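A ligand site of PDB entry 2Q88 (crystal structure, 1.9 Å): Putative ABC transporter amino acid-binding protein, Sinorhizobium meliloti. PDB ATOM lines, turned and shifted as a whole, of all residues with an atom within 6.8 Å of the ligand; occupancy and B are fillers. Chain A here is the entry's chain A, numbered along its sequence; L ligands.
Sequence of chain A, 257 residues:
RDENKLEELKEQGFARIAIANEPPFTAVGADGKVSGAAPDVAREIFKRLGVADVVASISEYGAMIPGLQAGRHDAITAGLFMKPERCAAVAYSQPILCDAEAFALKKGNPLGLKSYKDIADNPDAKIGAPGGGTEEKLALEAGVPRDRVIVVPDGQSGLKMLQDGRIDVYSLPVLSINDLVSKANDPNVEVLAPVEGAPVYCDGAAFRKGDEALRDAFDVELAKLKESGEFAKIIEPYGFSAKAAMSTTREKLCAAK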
ATOM      1  N   GLU A  22       3.629  14.956 -18.268  1.00  0.00           N
ATOM      2  CA  GLU A  22       3.673  13.648 -17.607  1.00  0.00           C
ATOM      3  C   GLU A  22       3.656  13.880 -16.093  1.00  0.00           C
ATOM      4  O   GLU A  22       4.714  13.947 -15.467  1.00  0.00           O
ATOM      5  CB  GLU A  22       4.930  12.864 -18.011  1.00  0.00           C
ATOM      6  CG  GLU A  22       5.032  11.477 -17.378  1.00  0.00           C
ATOM      7  CD  GLU A  22       6.356  10.790 -17.655  1.00  0.00           C
ATOM      8  OE1 GLU A  22       6.768  10.765 -18.829  1.00  0.00           O
ATOM      9  OE2 GLU A  22       6.993  10.270 -16.691  1.00  0.00           O
ATOM     10  N   PHE A  25       5.769  15.099 -12.920  1.00  0.00           N
ATOM     11  CA  PHE A  25       6.938  15.835 -13.393  1.00  0.00           C
ATOM     12  C   PHE A  25       6.542  17.144 -14.086  1.00  0.00           C
ATOM     13  O   PHE A  25       7.121  18.191 -13.809  1.00  0.00           O
ATOM     14  CB  PHE A  25       7.768  14.980 -14.354  1.00  0.00           C
ATOM     15  CG  PHE A  25       8.387  13.770 -13.708  1.00  0.00           C
ATOM     16  CD1 PHE A  25       7.674  12.597 -13.562  1.00  0.00           C
ATOM     17  CD2 PHE A  25       9.715  13.810 -13.262  1.00  0.00           C
ATOM     18  CE1 PHE A  25       8.255  11.459 -12.969  1.00  0.00           C
ATOM     19  CE2 PHE A  25      10.305  12.683 -12.682  1.00  0.00           C
ATOM     20  CZ  PHE A  25       9.575  11.508 -12.536  1.00  0.00           C
ATOM     21  N   TYR A  61      10.075  13.091 -25.554  1.00  0.00           N
ATOM     22  CA  TYR A  61      11.380  13.267 -24.904  1.00  0.00           C
ATOM     23  C   TYR A  61      12.531  13.293 -25.889  1.00  0.00           C
ATOM     24  O   TYR A  61      13.505  14.006 -25.687  1.00  0.00           O
ATOM     25  CB  TYR A  61      11.612  12.203 -23.820  1.00  0.00           C
ATOM     26  CG  TYR A  61      10.727  12.381 -22.615  1.00  0.00           C
ATOM     27  CD1 TYR A  61      11.089  13.242 -21.581  1.00  0.00           C
ATOM     28  CD2 TYR A  61       9.516  11.716 -22.509  1.00  0.00           C
ATOM     29  CE1 TYR A  61      10.258  13.418 -20.458  1.00  0.00           C
ATOM     30  CE2 TYR A  61       8.668  11.889 -21.385  1.00  0.00           C
ATOM     31  CZ  TYR A  61       9.067  12.734 -20.370  1.00  0.00           C
ATOM     32  OH  TYR A  61       8.240  12.917 -19.268  1.00  0.00           O
ATOM     33  N   ALA A  78      11.803  18.911 -17.482  1.00  0.00           N
ATOM     34  CA  ALA A  78      10.832  17.897 -17.863  1.00  0.00           C
ATOM     35  C   ALA A  78      11.006  16.564 -17.150  1.00  0.00           C
ATOM     36  O   ALA A  78      10.305  15.603 -17.465  1.00  0.00           O
ATOM     37  CB  ALA A  78      10.874  17.690 -19.383  1.00  0.00           C
ATOM     38  N   GLY A  79      11.922  16.488 -16.196  1.00  0.00           N
ATOM     39  CA  GLY A  79      12.297  15.207 -15.612  1.00  0.00           C
ATOM     40  C   GLY A  79      13.177  14.443 -16.580  1.00  0.00           C
ATOM     41  O   GLY A  79      13.107  13.205 -16.645  1.00  0.00           O
ATOM     42  N   LEU A  80      13.994  15.160 -17.352  1.00  0.00           N
ATOM     43  CA  LEU A  80      14.934  14.536 -18.293  1.00  0.00           C
ATOM     44  C   LEU A  80      16.155  14.031 -17.527  1.00  0.00           C
ATOM     45  O   LEU A  80      17.100  14.771 -17.248  1.00  0.00           O
ATOM     46  CB  LEU A  80      15.324  15.509 -19.418  1.00  0.00           C
ATOM     47  CG  LEU A  80      16.098  14.894 -20.596  1.00  0.00           C
ATOM     48  CD1 LEU A  80      15.196  14.079 -21.530  1.00  0.00           C
ATOM     49  CD2 LEU A  80      16.841  15.974 -21.362  1.00  0.00           C
ATOM     50  N   PHE A  81      16.109  12.749 -17.170  1.00  0.00           N
ATOM     51  CA  PHE A  81      17.053  12.156 -16.252  1.00  0.00           C
ATOM     52  C   PHE A  81      18.494  12.246 -16.751  1.00  0.00           C
ATOM     53  O   PHE A  81      18.744  12.084 -17.959  1.00  0.00           O
ATOM     54  CB  PHE A  81      16.717  10.680 -15.991  1.00  0.00           C
ATOM     55  CG  PHE A  81      15.375  10.460 -15.330  1.00  0.00           C
ATOM     56  CD1 PHE A  81      14.991  11.181 -14.195  1.00  0.00           C
ATOM     57  CD2 PHE A  81      14.530   9.442 -15.791  1.00  0.00           C
ATOM     58  CE1 PHE A  81      13.763  10.937 -13.566  1.00  0.00           C
ATOM     59  CE2 PHE A  81      13.285   9.194 -15.161  1.00  0.00           C
ATOM     60  CZ  PHE A  81      12.920   9.939 -14.054  1.00  0.00           C
ATOM     61  N   MET A  82      19.428  12.490 -15.838  1.00  0.00           N
ATOM     62  CA  MET A  82      20.850  12.600 -16.169  1.00  0.00           C
ATOM     63  C   MET A  82      21.446  11.255 -16.494  1.00  0.00           C
ATOM     64  O   MET A  82      21.223  10.282 -15.774  1.00  0.00           O
ATOM     65  CB  MET A  82      21.639  13.207 -15.017  1.00  0.00           C
ATOM     66  CG  MET A  82      21.181  14.599 -14.603  1.00  0.00           C
ATOM     67  SD  MET A  82      22.452  15.372 -13.558  1.00  0.00           S
ATOM     68  CE  MET A  82      21.444  16.571 -12.722  1.00  0.00           C
ATOM     69  N   LYS A  83      22.227  11.220 -17.574  1.00  0.00           N
ATOM     70  CA  LYS A  83      22.946  10.048 -18.023  1.00  0.00           C
ATOM     71  C   LYS A  83      24.192  10.523 -18.740  1.00  0.00           C
ATOM     72  O   LYS A  83      24.172  11.580 -19.362  1.00  0.00           O
ATOM     73  CB  LYS A  83      22.122   9.238 -19.033  1.00  0.00           C
ATOM     74  CG  LYS A  83      20.845   8.640 -18.500  1.00  0.00           C
ATOM     75  CD  LYS A  83      19.889   8.391 -19.654  1.00  0.00           C
ATOM     76  CE  LYS A  83      20.302   7.187 -20.470  1.00  0.00           C
ATOM     77  NZ  LYS A  83      19.281   6.896 -21.510  1.00  0.00           N
ATOM     78  N   ARG A  86      23.641  12.016 -22.170  1.00  0.00           N
ATOM     79  CA  ARG A  86      22.915  13.275 -22.139  1.00  0.00           C
ATOM     80  C   ARG A  86      23.790  14.369 -21.549  1.00  0.00           C
ATOM     81  O   ARG A  86      23.756  15.495 -22.018  1.00  0.00           O
ATOM     82  CB  ARG A  86      21.640  13.131 -21.309  1.00  0.00           C
ATOM     83  CG  ARG A  86      20.624  12.162 -21.874  1.00  0.00           C
ATOM     84  CD  ARG A  86      19.376  12.049 -20.999  1.00  0.00           C
ATOM     85  NE  ARG A  86      18.351  11.225 -21.625  1.00  0.00           N
ATOM     86  CZ  ARG A  86      17.179  10.936 -21.069  1.00  0.00           C
ATOM     87  NH1 ARG A  86      16.867  11.376 -19.859  1.00  0.00           N
ATOM     88  NH2 ARG A  86      16.316  10.181 -21.748  1.00  0.00           N
ATOM     89  N   TYR A  92      23.786  20.478 -17.517  1.00  0.00           N
ATOM     90  CA  TYR A  92      22.804  20.185 -16.483  1.00  0.00           C
ATOM     91  C   TYR A  92      23.032  21.000 -15.224  1.00  0.00           C
ATOM     92  O   TYR A  92      24.176  21.285 -14.857  1.00  0.00           O
ATOM     93  CB  TYR A  92      22.884  18.709 -16.088  1.00  0.00           C
ATOM     94  CG  TYR A  92      21.958  17.768 -16.849  1.00  0.00           C
ATOM     95  CD1 TYR A  92      20.580  17.833 -16.693  1.00  0.00           C
ATOM     96  CD2 TYR A  92      22.491  16.765 -17.664  1.00  0.00           C
ATOM     97  CE1 TYR A  92      19.733  16.939 -17.375  1.00  0.00           C
ATOM     98  CE2 TYR A  92      21.666  15.879 -18.354  1.00  0.00           C
ATOM     99  CZ  TYR A  92      20.300  15.973 -18.210  1.00  0.00           C
ATOM    100  OH  TYR A  92      19.492  15.100 -18.878  1.00  0.00           O
ATOM    101  N   GLU A 101      11.992   3.421 -11.785  1.00  0.00           N
ATOM    102  CA  GLU A 101      11.156   3.078 -12.938  1.00  0.00           C
ATOM    103  C   GLU A 101      10.091   2.073 -12.519  1.00  0.00           C
ATOM    104  O   GLU A 101      10.320   1.264 -11.604  1.00  0.00           O
ATOM    105  CB  GLU A 101      11.992   2.489 -14.082  1.00  0.00           C
ATOM    106  CG  GLU A 101      13.165   3.353 -14.547  1.00  0.00           C
ATOM    107  CD  GLU A 101      12.730   4.449 -15.506  1.00  0.00           C
ATOM    108  OE1 GLU A 101      11.564   4.889 -15.420  1.00  0.00           O
ATOM    109  OE2 GLU A 101      13.540   4.852 -16.371  1.00  0.00           O
ATOM    110  N   PRO A 130       7.926   5.953 -23.694  1.00  0.00           N
ATOM    111  CA  PRO A 130       8.133   7.208 -24.422  1.00  0.00           C
ATOM    112  C   PRO A 130       9.368   7.142 -25.310  1.00  0.00           C
ATOM    113  O   PRO A 130      10.405   6.609 -24.898  1.00  0.00           O
ATOM    114  CB  PRO A 130       8.281   8.256 -23.314  1.00  0.00           C
ATOM    115  CG  PRO A 130       8.584   7.498 -22.070  1.00  0.00           C
ATOM    116  CD  PRO A 130       7.955   6.140 -22.231  1.00  0.00           C
ATOM    117  N   GLY A 131       9.252   7.655 -26.533  1.00  0.00           N
ATOM    118  CA  GLY A 131      10.350   7.652 -27.489  1.00  0.00           C
ATOM    119  C   GLY A 131      11.472   8.556 -27.011  1.00  0.00           C
ATOM    120  O   GLY A 131      11.226   9.687 -26.586  1.00  0.00           O
ATOM    121  N   GLY A 132      12.702   8.049 -27.080  1.00  0.00           N
ATOM    122  CA  GLY A 132      13.887   8.776 -26.606  1.00  0.00           C
ATOM    123  C   GLY A 132      14.027   8.795 -25.093  1.00  0.00           C
ATOM    124  O   GLY A 132      14.876   9.520 -24.552  1.00  0.00           O
ATOM    125  N   GLY A 133      13.203   8.017 -24.407  1.00  0.00           N
ATOM    126  CA  GLY A 133      13.172   7.992 -22.944  1.00  0.00           C
ATOM    127  C   GLY A 133      14.095   6.957 -22.327  1.00  0.00           C
ATOM    128  O   GLY A 133      14.527   6.011 -22.999  1.00  0.00           O
ATOM    129  N   THR A 134      14.367   7.104 -21.029  1.00  0.00           N
ATOM    130  CA  THR A 134      15.203   6.134 -20.313  1.00  0.00           C
ATOM    131  C   THR A 134      14.640   4.733 -20.348  1.00  0.00           C
ATOM    132  O   THR A 134      15.410   3.776 -20.417  1.00  0.00           O
ATOM    133  CB  THR A 134      15.431   6.542 -18.838  1.00  0.00           C
ATOM    134  OG1 THR A 134      14.180   6.945 -18.251  1.00  0.00           O
ATOM    135  CG2 THR A 134      16.321   7.786 -18.745  1.00  0.00           C
ATOM    136  N   GLU A 135      13.322   4.586 -20.257  1.00  0.00           N
ATOM    137  CA  GLU A 135      12.724   3.239 -20.241  1.00  0.00           C
ATOM    138  C   GLU A 135      12.950   2.526 -21.563  1.00  0.00           C
ATOM    139  O   GLU A 135      13.279   1.342 -21.579  1.00  0.00           O
ATOM    140  CB  GLU A 135      11.220   3.286 -19.964  1.00  0.00           C
ATOM    141  CG  GLU A 135      10.879   3.913 -18.630  1.00  0.00           C
ATOM    142  CD  GLU A 135      10.933   5.429 -18.694  1.00  0.00           C
ATOM    143  OE1 GLU A 135      10.918   5.964 -19.814  1.00  0.00           O
ATOM    144  OE2 GLU A 135      10.981   6.062 -17.622  1.00  0.00           O
ATOM    145  N   SER A 171       5.899   1.366 -19.424  1.00  0.00           N
ATOM    146  CA  SER A 171       6.890   1.751 -18.441  1.00  0.00           C
ATOM    147  C   SER A 171       7.095   3.268 -18.402  1.00  0.00           C
ATOM    148  O   SER A 171       7.305   3.892 -19.428  1.00  0.00           O
ATOM    149  CB  SER A 171       8.210   1.050 -18.733  1.00  0.00           C
ATOM    150  OG  SER A 171       9.139   1.293 -17.692  1.00  0.00           O
ATOM    151  N   LEU A 172       6.996   3.814 -17.180  1.00  0.00           N
ATOM    152  CA  LEU A 172       7.287   5.217 -16.840  1.00  0.00           C
ATOM    153  C   LEU A 172       7.899   5.211 -15.442  1.00  0.00           C
ATOM    154  O   LEU A 172       7.914   4.158 -14.791  1.00  0.00           O
ATOM    155  CB  LEU A 172       5.986   6.043 -16.813  1.00  0.00           C
ATOM    156  CG  LEU A 172       5.309   6.448 -18.122  1.00  0.00           C
ATOM    157  CD1 LEU A 172       4.140   7.340 -17.832  1.00  0.00           C
ATOM    158  CD2 LEU A 172       6.280   7.136 -19.066  1.00  0.00           C
ATOM    159  N   PRO A 173       8.398   6.353 -14.962  1.00  0.00           N
ATOM    160  CA  PRO A 173       8.770   6.492 -13.558  1.00  0.00           C
ATOM    161  C   PRO A 173       7.631   6.131 -12.600  1.00  0.00           C
ATOM    162  O   PRO A 173       6.472   6.357 -12.911  1.00  0.00           O
ATOM    163  CB  PRO A 173       9.143   7.976 -13.450  1.00  0.00           C
ATOM    164  CG  PRO A 173       9.638   8.320 -14.800  1.00  0.00           C
ATOM    165  CD  PRO A 173       8.675   7.598 -15.725  1.00  0.00           C
ATOM    166  N   SER A 176       4.928   8.676 -11.974  1.00  0.00           N
ATOM    167  CA  SER A 176       4.094   8.892 -13.167  1.00  0.00           C
ATOM    168  C   SER A 176       3.087   7.755 -13.381  1.00  0.00           C
ATOM    169  O   SER A 176       1.929   8.003 -13.733  1.00  0.00           O
ATOM    170  CB  SER A 176       4.950   9.021 -14.426  1.00  0.00           C
ATOM    171  OG  SER A 176       5.923  10.046 -14.315  1.00  0.00           O
ATOM    172  N   TYR A 201      17.085   7.121 -11.147  1.00  0.00           N
ATOM    173  CA  TYR A 201      17.578   8.264 -11.894  1.00  0.00           C
ATOM    174  C   TYR A 201      17.214   9.543 -11.144  1.00  0.00           C
ATOM    175  O   TYR A 201      16.284   9.542 -10.342  1.00  0.00           O
ATOM    176  CB  TYR A 201      16.887   8.330 -13.265  1.00  0.00           C
ATOM    177  CG  TYR A 201      17.317   7.290 -14.270  1.00  0.00           C
ATOM    178  CD1 TYR A 201      18.569   7.356 -14.872  1.00  0.00           C
ATOM    179  CD2 TYR A 201      16.454   6.267 -14.645  1.00  0.00           C
ATOM    180  CE1 TYR A 201      18.964   6.410 -15.806  1.00  0.00           C
ATOM    181  CE2 TYR A 201      16.839   5.311 -15.580  1.00  0.00           C
ATOM    182  CZ  TYR A 201      18.101   5.396 -16.159  1.00  0.00           C
ATOM    183  OH  TYR A 201      18.497   4.448 -17.079  1.00  0.00           O
ATOM    184  N   ASP A 203      16.842  13.874 -12.340  1.00  0.00           N
ATOM    185  CA  ASP A 203      16.949  14.881 -13.390  1.00  0.00           C
ATOM    186  C   ASP A 203      17.655  16.154 -12.910  1.00  0.00           C
ATOM    187  O   ASP A 203      18.127  16.245 -11.776  1.00  0.00           O
ATOM    188  CB  ASP A 203      15.557  15.199 -13.974  1.00  0.00           C
ATOM    189  CG  ASP A 203      14.857  16.337 -13.246  1.00  0.00           C
ATOM    190  OD1 ASP A 203      15.142  16.588 -12.058  1.00  0.00           O
ATOM    191  OD2 ASP A 203      14.003  17.064 -13.812  1.00  0.00           O
HETATM  192  O1  LIG L   1      13.949   9.747 -20.397  1.00  0.00           O
HETATM  193  C1  LIG L   1      13.581  10.305 -19.361  1.00  0.00           C
HETATM  194  O2  LIG L   1      14.266  11.202 -18.860  1.00  0.00           O
HETATM  195  C2  LIG L   1      12.285   9.873 -18.686  1.00  0.00           C
HETATM  196  C3  LIG L   1      11.166   9.560 -19.665  1.00  0.00           C
HETATM  197  C4  LIG L   1       9.923   9.090 -18.897  1.00  0.00           C
HETATM  198  N1  LIG L   1       9.541  10.121 -17.897  1.00  0.00           N
HETATM  199  C5  LIG L   1      10.505  10.981 -17.327  1.00  0.00           C
HETATM  200  C6  LIG L   1      10.085  12.040 -16.299  1.00  0.00           C
HETATM  201  N2  LIG L   1      11.845  10.895 -17.718  1.00  0.00           N
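OE2 of Glu 22 is in hydrogen-bond range of N1 of the ligand, at 2.8 Å. An oxygen (O1) of the ligand is in salt-bridge range of the guanidinium group (NH2) of Arg 86 (2.8 Å). OH of Tyr 61 lies within hydrogen-bond range of N1 of the ligand (3.4 Å). O of Gly 79 sits close to N2 of the ligand (2.8 Å). The backbone NH (N) of Phe 81 sits at hydrogen-bond distance from an oxygen (O2) of the ligand (2.9 Å). The backbone NH (N) of Thr 134 sits at hydrogen-bond distance from an oxygen (O1) of the ligand (2.7 Å).
CD2 of Phe 25 touches C6 of the ligand, at 3.5 Å. Ala 78 touches the ligand. Leu 80 touches the ligand (CA to O2, 3.4 Å). CG of Pro 130 touches C4 of the ligand, at 3.8 Å. Gly 133 touches the ligand (CA to O1, 3.2 Å). Glu 135 touches the ligand (OE1 to C4, 3.4 Å). Pro 173 touches the ligand (CD to N1, 3.4 Å). Hydrophobic or aromatic side chains within 4 Å of the ligand: Phe 25, Tyr 61, Phe 81, Pro 130 and Pro 173. 13 residues have an atom within 4 Å of the ligand: Glu 22, Phe 25, Tyr 61, Ala 78, Gly 79, Leu 80, Phe 81, Arg 86, Pro 130, Gly 133, Thr 134, Glu 135 and Pro 173. The nearest printed residue that does not touch the ligand is Leu 172 (4.1 Å).
The side-chain hydroxyl of Tyr 92 sits at hydrogen-bond distance from the backbone carbonyl oxygen of Phe 81. The side-chain carboxylate (OE1) of Glu 101 sits close to the side-chain carboxylate (OE2) of Glu 135 (2.6 Å). The side-chain hydroxyl (OG) of Ser 176 lies within hydrogen-bond range of the side-chain carboxylate (OE2) of Glu 22, at 2.6 Å. The side-chain carboxylate of Asp 203 lies close to the backbone NH of Gly 79, at 3.2 Å. The side-chain carboxylate (OE1) of Glu 22 lies within hydrogen-bond range of the side-chain hydroxyl (OH) of Tyr 61, at 2.6 Å. The guanidinium group (NH1) of Arg 86 is in hydrogen-bond range of the backbone carbonyl oxygen (O) of Phe 81 (2.8 Å). The guanidinium group of Arg 86 lies within hydrogen-bond range of the backbone carbonyl oxygen of Gly 132. The side-chain hydroxyl of Thr 134 is in hydrogen-bond range of the side-chain carboxylate of Glu 135 (3.4 Å).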
